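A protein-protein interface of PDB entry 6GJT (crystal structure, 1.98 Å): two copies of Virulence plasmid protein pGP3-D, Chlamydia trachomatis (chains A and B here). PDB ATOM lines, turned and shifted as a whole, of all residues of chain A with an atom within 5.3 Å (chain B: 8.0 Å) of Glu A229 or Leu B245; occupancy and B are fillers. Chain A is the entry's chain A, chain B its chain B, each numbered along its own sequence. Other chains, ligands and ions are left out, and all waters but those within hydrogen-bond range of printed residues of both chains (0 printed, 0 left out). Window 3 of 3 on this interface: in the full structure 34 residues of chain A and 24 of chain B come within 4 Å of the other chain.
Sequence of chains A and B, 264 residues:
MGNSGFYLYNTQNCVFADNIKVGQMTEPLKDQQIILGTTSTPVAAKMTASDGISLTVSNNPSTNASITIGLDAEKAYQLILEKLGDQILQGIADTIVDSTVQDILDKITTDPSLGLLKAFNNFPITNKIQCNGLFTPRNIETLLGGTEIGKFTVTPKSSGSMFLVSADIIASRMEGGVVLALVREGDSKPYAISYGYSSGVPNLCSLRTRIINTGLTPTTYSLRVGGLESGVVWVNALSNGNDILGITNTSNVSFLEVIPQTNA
The side-chain hydroxyl (OH) of Tyr A195 sits at hydrogen-bond distance from the side-chain amide oxygen (OD1) of Asn B249 (2.7 Å).
The backbone NH (N) of Phe A135 is in hydrogen-bond range of the backbone carbonyl oxygen (O) of Gly A227 (2.8 Å).
The backbone NH (N) of Glu A229 sits at hydrogen-bond distance from the backbone carbonyl oxygen (O) of Phe A135 (2.8 Å).
ND2 of Asn B249 is in hydrogen-bond range of O of Ile B244.
The backbone carbonyl oxygen (O) of Ile B247 is in hydrogen-bond range of the side-chain amide nitrogen (ND2) of Asn B249 (3.4 Å).
Thr A136 touches Leu B245.
CA of Pro A137 touches O of Leu B245, at 3.6 Å.
O of Leu B245 touches CG2 of Ile A140 (3.4 Å).
Ile A140 touches Ile B247 (CG1 to CD1, 3.8 Å).
Pro B202 touches Tyr A195 (O to CB, 3.7 Å).
CG2 of Ile B244 touches OH of Tyr A195, at 3.5 Å.
Tyr A195 touches Leu B245.
Leu A228 touches Pro B202 (CD2 to CD, 3.99 Å).
Leu A228 touches Leu B245.
CD2 of Leu B245 touches OE2 of Glu A229, 3.8 Å away.
Of the printed residues of chain B, Thr A136 touches Leu B245 (3.7 Å).
Of the printed residues of chain B, Ile A140 touches Leu B245 and Ile B247.
Of the printed residues of chain B, Tyr A195 touches Pro B202 (3.7 Å), Ile B244 (3.5 Å), Leu B245 (3.9 Å) and Asn B249 (2.7 Å).
Printed residues of chain A within 4 Å of Pro B202: Tyr A195 (3.7 Å) and Leu A228 (3.99 Å).
Leu B238 touches none of the printed residues of chain A.
Leu B245 touches just these residues of chain A: Phe A135 (3.9 Å), Thr A136 (3.7 Å), Pro A137 (3.6 Å), Ile A140 (3.4 Å), Tyr A195 (3.9 Å), Leu A228 (3.9 Å) and Glu A229 (3.8 Å).
Of the printed residues of chain A, Ile B247 touches Ile A140.
The nearest residue of chain A that does not touch Leu B245 is Val A179 (4.4 Å).
Of the 12 printed residues of chain B, 5 touch a printed residue of chain A.
Of the 12 printed residues of chain A, 7 touch a printed residue of chain B.
Among the printed residues, 12 pairs touch across the chains.
Among the printed residues, no Asp or Glu carboxylate lies within 4 Å of a Lys or Arg side-chain nitrogen of the other chain.
No position is printed for both chains.
Of the 12 pairs that touch across the chains among the printed residues, none has its exchanged pair printed and touching as well.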
ATOM      1  N   LEU A 134      34.716  28.338  11.489  1.00  0.00           N
ATOM      2  CA  LEU A 134      33.794  27.478  12.245  1.00  0.00           C
ATOM      3  C   LEU A 134      33.634  28.086  13.643  1.00  0.00           C
ATOM      4  O   LEU A 134      34.491  28.843  14.111  1.00  0.00           O
ATOM      5  CB  LEU A 134      34.380  26.080  12.348  1.00  0.00           C
ATOM      6  CG  LEU A 134      34.468  25.324  11.016  1.00  0.00           C
ATOM      7  CD1 LEU A 134      35.252  24.040  11.221  1.00  0.00           C
ATOM      8  CD2 LEU A 134      33.076  25.026  10.497  1.00  0.00           C
ATOM      9  N   PHE A 135      32.538  27.741  14.307  1.00  0.00           N
ATOM     10  CA  PHE A 135      32.474  27.902  15.727  1.00  0.00           C
ATOM     11  C   PHE A 135      32.645  26.552  16.420  1.00  0.00           C
ATOM     12  O   PHE A 135      31.990  25.560  16.092  1.00  0.00           O
ATOM     13  CB  PHE A 135      31.162  28.603  16.131  1.00  0.00           C
ATOM     14  CG  PHE A 135      31.168  30.070  15.869  1.00  0.00           C
ATOM     15  CD1 PHE A 135      31.773  30.933  16.754  1.00  0.00           C
ATOM     16  CD2 PHE A 135      30.528  30.608  14.752  1.00  0.00           C
ATOM     17  CE1 PHE A 135      31.757  32.267  16.556  1.00  0.00           C
ATOM     18  CE2 PHE A 135      30.466  31.970  14.567  1.00  0.00           C
ATOM     19  CZ  PHE A 135      31.121  32.812  15.453  1.00  0.00           C
ATOM     20  N   THR A 136      33.545  26.504  17.395  1.00  0.00           N
ATOM     21  CA  THR A 136      33.842  25.291  18.126  1.00  0.00           C
ATOM     22  C   THR A 136      34.036  25.624  19.584  1.00  0.00           C
ATOM     23  O   THR A 136      34.149  26.811  19.955  1.00  0.00           O
ATOM     24  CB  THR A 136      35.214  24.675  17.708  1.00  0.00           C
ATOM     25  OG1 THR A 136      36.257  25.544  18.152  1.00  0.00           O
ATOM     26  CG2 THR A 136      35.309  24.491  16.235  1.00  0.00           C
ATOM     27  N   PRO A 137      34.084  24.582  20.448  1.00  0.00           N
ATOM     28  CA  PRO A 137      34.233  24.921  21.888  1.00  0.00           C
ATOM     29  C   PRO A 137      35.561  25.651  22.173  1.00  0.00           C
ATOM     30  O   PRO A 137      35.667  26.422  23.113  1.00  0.00           O
ATOM     31  CB  PRO A 137      34.226  23.540  22.595  1.00  0.00           C
ATOM     32  CG  PRO A 137      33.565  22.609  21.648  1.00  0.00           C
ATOM     33  CD  PRO A 137      33.868  23.142  20.247  1.00  0.00           C
ATOM     34  N   ILE A 140      34.827  29.500  20.737  1.00  0.00           N
ATOM     35  CA  ILE A 140      33.589  30.223  20.991  1.00  0.00           C
ATOM     36  C   ILE A 140      33.763  31.409  21.948  1.00  0.00           C
ATOM     37  O   ILE A 140      33.150  32.460  21.745  1.00  0.00           O
ATOM     38  CB  ILE A 140      32.466  29.298  21.484  1.00  0.00           C
ATOM     39  CG1 ILE A 140      31.141  30.063  21.604  1.00  0.00           C
ATOM     40  CG2 ILE A 140      32.823  28.612  22.798  1.00  0.00           C
ATOM     41  CD1 ILE A 140      30.649  30.673  20.302  1.00  0.00           C
ATOM     42  N   VAL A 179      25.857  29.377  13.528  1.00  0.00           N
ATOM     43  CA  VAL A 179      26.094  30.146  14.750  1.00  0.00           C
ATOM     44  C   VAL A 179      26.306  31.575  14.419  1.00  0.00           C
ATOM     45  O   VAL A 179      26.931  31.887  13.431  1.00  0.00           O
ATOM     46  CB  VAL A 179      27.322  29.579  15.517  1.00  0.00           C
ATOM     47  CG1 VAL A 179      27.591  30.371  16.773  1.00  0.00           C
ATOM     48  CG2 VAL A 179      27.091  28.133  15.883  1.00  0.00           C
ATOM     49  N   TYR A 195      21.730  30.961  17.445  1.00  0.00           N
ATOM     50  CA  TYR A 195      21.882  29.748  16.663  1.00  0.00           C
ATOM     51  C   TYR A 195      20.796  29.724  15.603  1.00  0.00           C
ATOM     52  O   TYR A 195      19.679  30.158  15.816  1.00  0.00           O
ATOM     53  CB  TYR A 195      21.758  28.475  17.509  1.00  0.00           C
ATOM     54  CG  TYR A 195      22.812  28.379  18.525  1.00  0.00           C
ATOM     55  CD1 TYR A 195      22.730  29.127  19.676  1.00  0.00           C
ATOM     56  CD2 TYR A 195      24.006  27.769  18.267  1.00  0.00           C
ATOM     57  CE1 TYR A 195      23.757  29.164  20.610  1.00  0.00           C
ATOM     58  CE2 TYR A 195      25.045  27.804  19.238  1.00  0.00           C
ATOM     59  CZ  TYR A 195      24.922  28.556  20.395  1.00  0.00           C
ATOM     60  OH  TYR A 195      25.902  28.587  21.375  1.00  0.00           O
ATOM     61  N   GLY A 227      29.610  27.894  10.727  1.00  0.00           N
ATOM     62  CA  GLY A 227      29.036  26.613  11.064  1.00  0.00           C
ATOM     63  C   GLY A 227      29.198  26.215  12.536  1.00  0.00           C
ATOM     64  O   GLY A 227      30.228  26.526  13.195  1.00  0.00           O
ATOM     65  N   LEU A 228      28.222  25.482  13.028  1.00  0.00           N
ATOM     66  CA  LEU A 228      28.312  24.860  14.327  1.00  0.00           C
ATOM     67  C   LEU A 228      29.176  23.633  14.211  1.00  0.00           C
ATOM     68  O   LEU A 228      28.748  22.655  13.684  1.00  0.00           O
ATOM     69  CB  LEU A 228      26.909  24.505  14.839  1.00  0.00           C
ATOM     70  CG  LEU A 228      26.835  23.778  16.188  1.00  0.00           C
ATOM     71  CD1 LEU A 228      27.255  24.689  17.311  1.00  0.00           C
ATOM     72  CD2 LEU A 228      25.428  23.272  16.442  1.00  0.00           C
ATOM     73  N   GLU A 229      30.437  23.715  14.655  1.00  0.00           N
ATOM     74  CA  GLU A 229      31.403  22.576  14.662  1.00  0.00           C
ATOM     75  C   GLU A 229      31.962  22.251  13.282  1.00  0.00           C
ATOM     76  O   GLU A 229      33.126  21.952  13.177  1.00  0.00           O
ATOM     77  CB  GLU A 229      30.848  21.277  15.246  1.00  0.00           C
ATOM     78  CG  GLU A 229      30.313  21.344  16.679  1.00  0.00           C
ATOM     79  CD  GLU A 229      31.393  21.194  17.739  1.00  0.00           C
ATOM     80  OE1 GLU A 229      32.542  20.862  17.400  1.00  0.00           O
ATOM     81  OE2 GLU A 229      31.103  21.453  18.921  1.00  0.00           O
ATOM     82  N   SER A 230      31.133  22.221  12.250  1.00  0.00           N
ATOM     83  CA  SER A 230      31.610  21.951  10.919  1.00  0.00           C
ATOM     84  C   SER A 230      30.655  22.496   9.865  1.00  0.00           C
ATOM     85  O   SER A 230      29.555  22.931  10.185  1.00  0.00           O
ATOM     86  CB  SER A 230      31.792  20.439  10.693  1.00  0.00           C
ATOM     87  OG  SER A 230      30.577  19.774  10.831  1.00  0.00           O
ATOM     88  N   GLY A 231      31.116  22.522   8.640  1.00  0.00           N
ATOM     89  CA  GLY A 231      30.354  22.959   7.472  1.00  0.00           C
ATOM     90  C   GLY A 231      30.657  24.401   7.101  1.00  0.00           C
ATOM     91  O   GLY A 231      30.985  25.199   7.946  1.00  0.00           O
ATOM     92  N   VAL B 201      20.148  19.688  16.538  1.00  0.00           N
ATOM     93  CA  VAL B 201      21.093  20.618  17.023  1.00  0.00           C
ATOM     94  C   VAL B 201      20.308  21.935  17.428  1.00  0.00           C
ATOM     95  O   VAL B 201      19.211  22.260  16.950  1.00  0.00           O
ATOM     96  CB  VAL B 201      22.207  20.926  16.009  1.00  0.00           C
ATOM     97  CG1 VAL B 201      22.985  19.638  15.622  1.00  0.00           C
ATOM     98  CG2 VAL B 201      21.656  21.553  14.749  1.00  0.00           C
ATOM     99  N   PRO B 202      20.915  22.728  18.257  1.00  0.00           N
ATOM    100  CA  PRO B 202      20.170  23.940  18.786  1.00  0.00           C
ATOM    101  C   PRO B 202      19.783  24.967  17.685  1.00  0.00           C
ATOM    102  O   PRO B 202      20.499  25.118  16.688  1.00  0.00           O
ATOM    103  CB  PRO B 202      21.178  24.619  19.678  1.00  0.00           C
ATOM    104  CG  PRO B 202      22.256  23.676  19.891  1.00  0.00           C
ATOM    105  CD  PRO B 202      22.271  22.629  18.792  1.00  0.00           C
ATOM    106  N   ALA B 237      20.443  24.289  25.764  1.00  0.00           N
ATOM    107  CA  ALA B 237      21.301  23.182  25.896  1.00  0.00           C
ATOM    108  C   ALA B 237      21.150  22.319  24.632  1.00  0.00           C
ATOM    109  O   ALA B 237      20.307  22.562  23.829  1.00  0.00           O
ATOM    110  CB  ALA B 237      20.949  22.410  27.159  1.00  0.00           C
ATOM    111  N   LEU B 238      22.062  21.358  24.453  1.00  0.00           N
ATOM    112  CA  LEU B 238      22.011  20.331  23.421  1.00  0.00           C
ATOM    113  C   LEU B 238      20.923  19.343  23.762  1.00  0.00           C
ATOM    114  O   LEU B 238      20.396  19.388  24.846  1.00  0.00           O
ATOM    115  CB  LEU B 238      23.369  19.569  23.311  1.00  0.00           C
ATOM    116  CG  LEU B 238      24.622  20.393  22.968  1.00  0.00           C
ATOM    117  CD1 LEU B 238      25.937  19.576  23.112  1.00  0.00           C
ATOM    118  CD2 LEU B 238      24.523  21.013  21.583  1.00  0.00           C
ATOM    119  N   ASN B 242      23.649  18.770  27.697  1.00  0.00           N
ATOM    120  CA  ASN B 242      24.949  19.393  27.834  1.00  0.00           C
ATOM    121  C   ASN B 242      24.991  20.800  27.296  1.00  0.00           C
ATOM    122  O   ASN B 242      24.132  21.193  26.468  1.00  0.00           O
ATOM    123  CB  ASN B 242      25.992  18.570  27.047  1.00  0.00           C
ATOM    124  CG  ASN B 242      26.261  17.206  27.695  1.00  0.00           C
ATOM    125  OD1 ASN B 242      25.814  16.918  28.804  1.00  0.00           O
ATOM    126  ND2 ASN B 242      27.042  16.406  27.032  1.00  0.00           N
ATOM    127  N   ASP B 243      25.977  21.549  27.749  1.00  0.00           N
ATOM    128  CA  ASP B 243      26.191  22.949  27.342  1.00  0.00           C
ATOM    129  C   ASP B 243      26.436  23.081  25.868  1.00  0.00           C
ATOM    130  O   ASP B 243      27.181  22.282  25.282  1.00  0.00           O
ATOM    131  CB  ASP B 243      27.390  23.566  28.072  1.00  0.00           C
ATOM    132  CG  ASP B 243      27.142  23.846  29.560  1.00  0.00           C
ATOM    133  OD1 ASP B 243      26.013  23.817  30.036  1.00  0.00           O
ATOM    134  OD2 ASP B 243      28.112  24.191  30.242  1.00  0.00           O
ATOM    135  N   ILE B 244      25.782  24.030  25.226  1.00  0.00           N
ATOM    136  CA  ILE B 244      26.089  24.223  23.763  1.00  0.00           C
ATOM    137  C   ILE B 244      27.480  24.883  23.618  1.00  0.00           C
ATOM    138  O   ILE B 244      27.732  25.926  24.201  1.00  0.00           O
ATOM    139  CB  ILE B 244      25.029  25.080  23.053  1.00  0.00           C
ATOM    140  CG1 ILE B 244      23.644  24.464  23.224  1.00  0.00           C
ATOM    141  CG2 ILE B 244      25.402  25.167  21.560  1.00  0.00           C
ATOM    142  CD1 ILE B 244      22.498  25.422  23.079  1.00  0.00           C
ATOM    143  N   LEU B 245      28.391  24.242  22.873  1.00  0.00           N
ATOM    144  CA  LEU B 245      29.744  24.743  22.691  1.00  0.00           C
ATOM    145  C   LEU B 245      30.485  24.987  24.037  1.00  0.00           C
ATOM    146  O   LEU B 245      31.460  25.718  24.074  1.00  0.00           O
ATOM    147  CB  LEU B 245      29.737  26.045  21.849  1.00  0.00           C
ATOM    148  CG  LEU B 245      29.325  25.910  20.380  1.00  0.00           C
ATOM    149  CD1 LEU B 245      29.149  27.246  19.706  1.00  0.00           C
ATOM    150  CD2 LEU B 245      30.343  25.111  19.600  1.00  0.00           C
ATOM    151  N   GLY B 246      30.024  24.319  25.112  1.00  0.00           N
ATOM    152  CA  GLY B 246      30.715  24.279  26.389  1.00  0.00           C
ATOM    153  C   GLY B 246      30.483  25.489  27.225  1.00  0.00           C
ATOM    154  O   GLY B 246      31.283  25.738  28.073  1.00  0.00           O
ATOM    155  N   ILE B 247      29.466  26.334  26.877  1.00  0.00           N
ATOM    156  CA  ILE B 247      29.321  27.671  27.559  1.00  0.00           C
ATOM    157  C   ILE B 247      27.931  27.833  28.007  1.00  0.00           C
ATOM    158  O   ILE B 247      27.075  27.021  27.635  1.00  0.00           O
ATOM    159  CB  ILE B 247      29.687  28.896  26.656  1.00  0.00           C
ATOM    160  CG1 ILE B 247      28.870  28.922  25.361  1.00  0.00           C
ATOM    161  CG2 ILE B 247      31.201  28.895  26.333  1.00  0.00           C
ATOM    162  CD1 ILE B 247      28.879  30.241  24.640  1.00  0.00           C
ATOM    163  N   THR B 248      27.670  28.885  28.804  1.00  0.00           N
ATOM    164  CA  THR B 248      26.311  29.135  29.089  1.00  0.00           C
ATOM    165  C   THR B 248      25.749  29.980  27.912  1.00  0.00           C
ATOM    166  O   THR B 248      26.423  30.871  27.386  1.00  0.00           O
ATOM    167  CB  THR B 248      26.066  29.812  30.434  1.00  0.00           C
ATOM    168  OG1 THR B 248      26.158  31.177  30.214  1.00  0.00           O
ATOM    169  CG2 THR B 248      26.993  29.419  31.483  1.00  0.00           C
ATOM    170  N   ASN B 249      24.518  29.704  27.506  1.00  0.00           N
ATOM    171  CA  ASN B 249      23.866  30.416  26.443  1.00  0.00           C
ATOM    172  C   ASN B 249      22.672  31.161  26.951  1.00  0.00           C
ATOM    173  O   ASN B 249      22.216  30.878  28.064  1.00  0.00           O
ATOM    174  CB  ASN B 249      23.485  29.516  25.343  1.00  0.00           C
ATOM    175  CG  ASN B 249      24.690  29.114  24.529  1.00  0.00           C
ATOM    176  OD1 ASN B 249      25.099  29.829  23.602  1.00  0.00           O
ATOM    177  ND2 ASN B 249      25.290  28.000  24.874  1.00  0.00           N
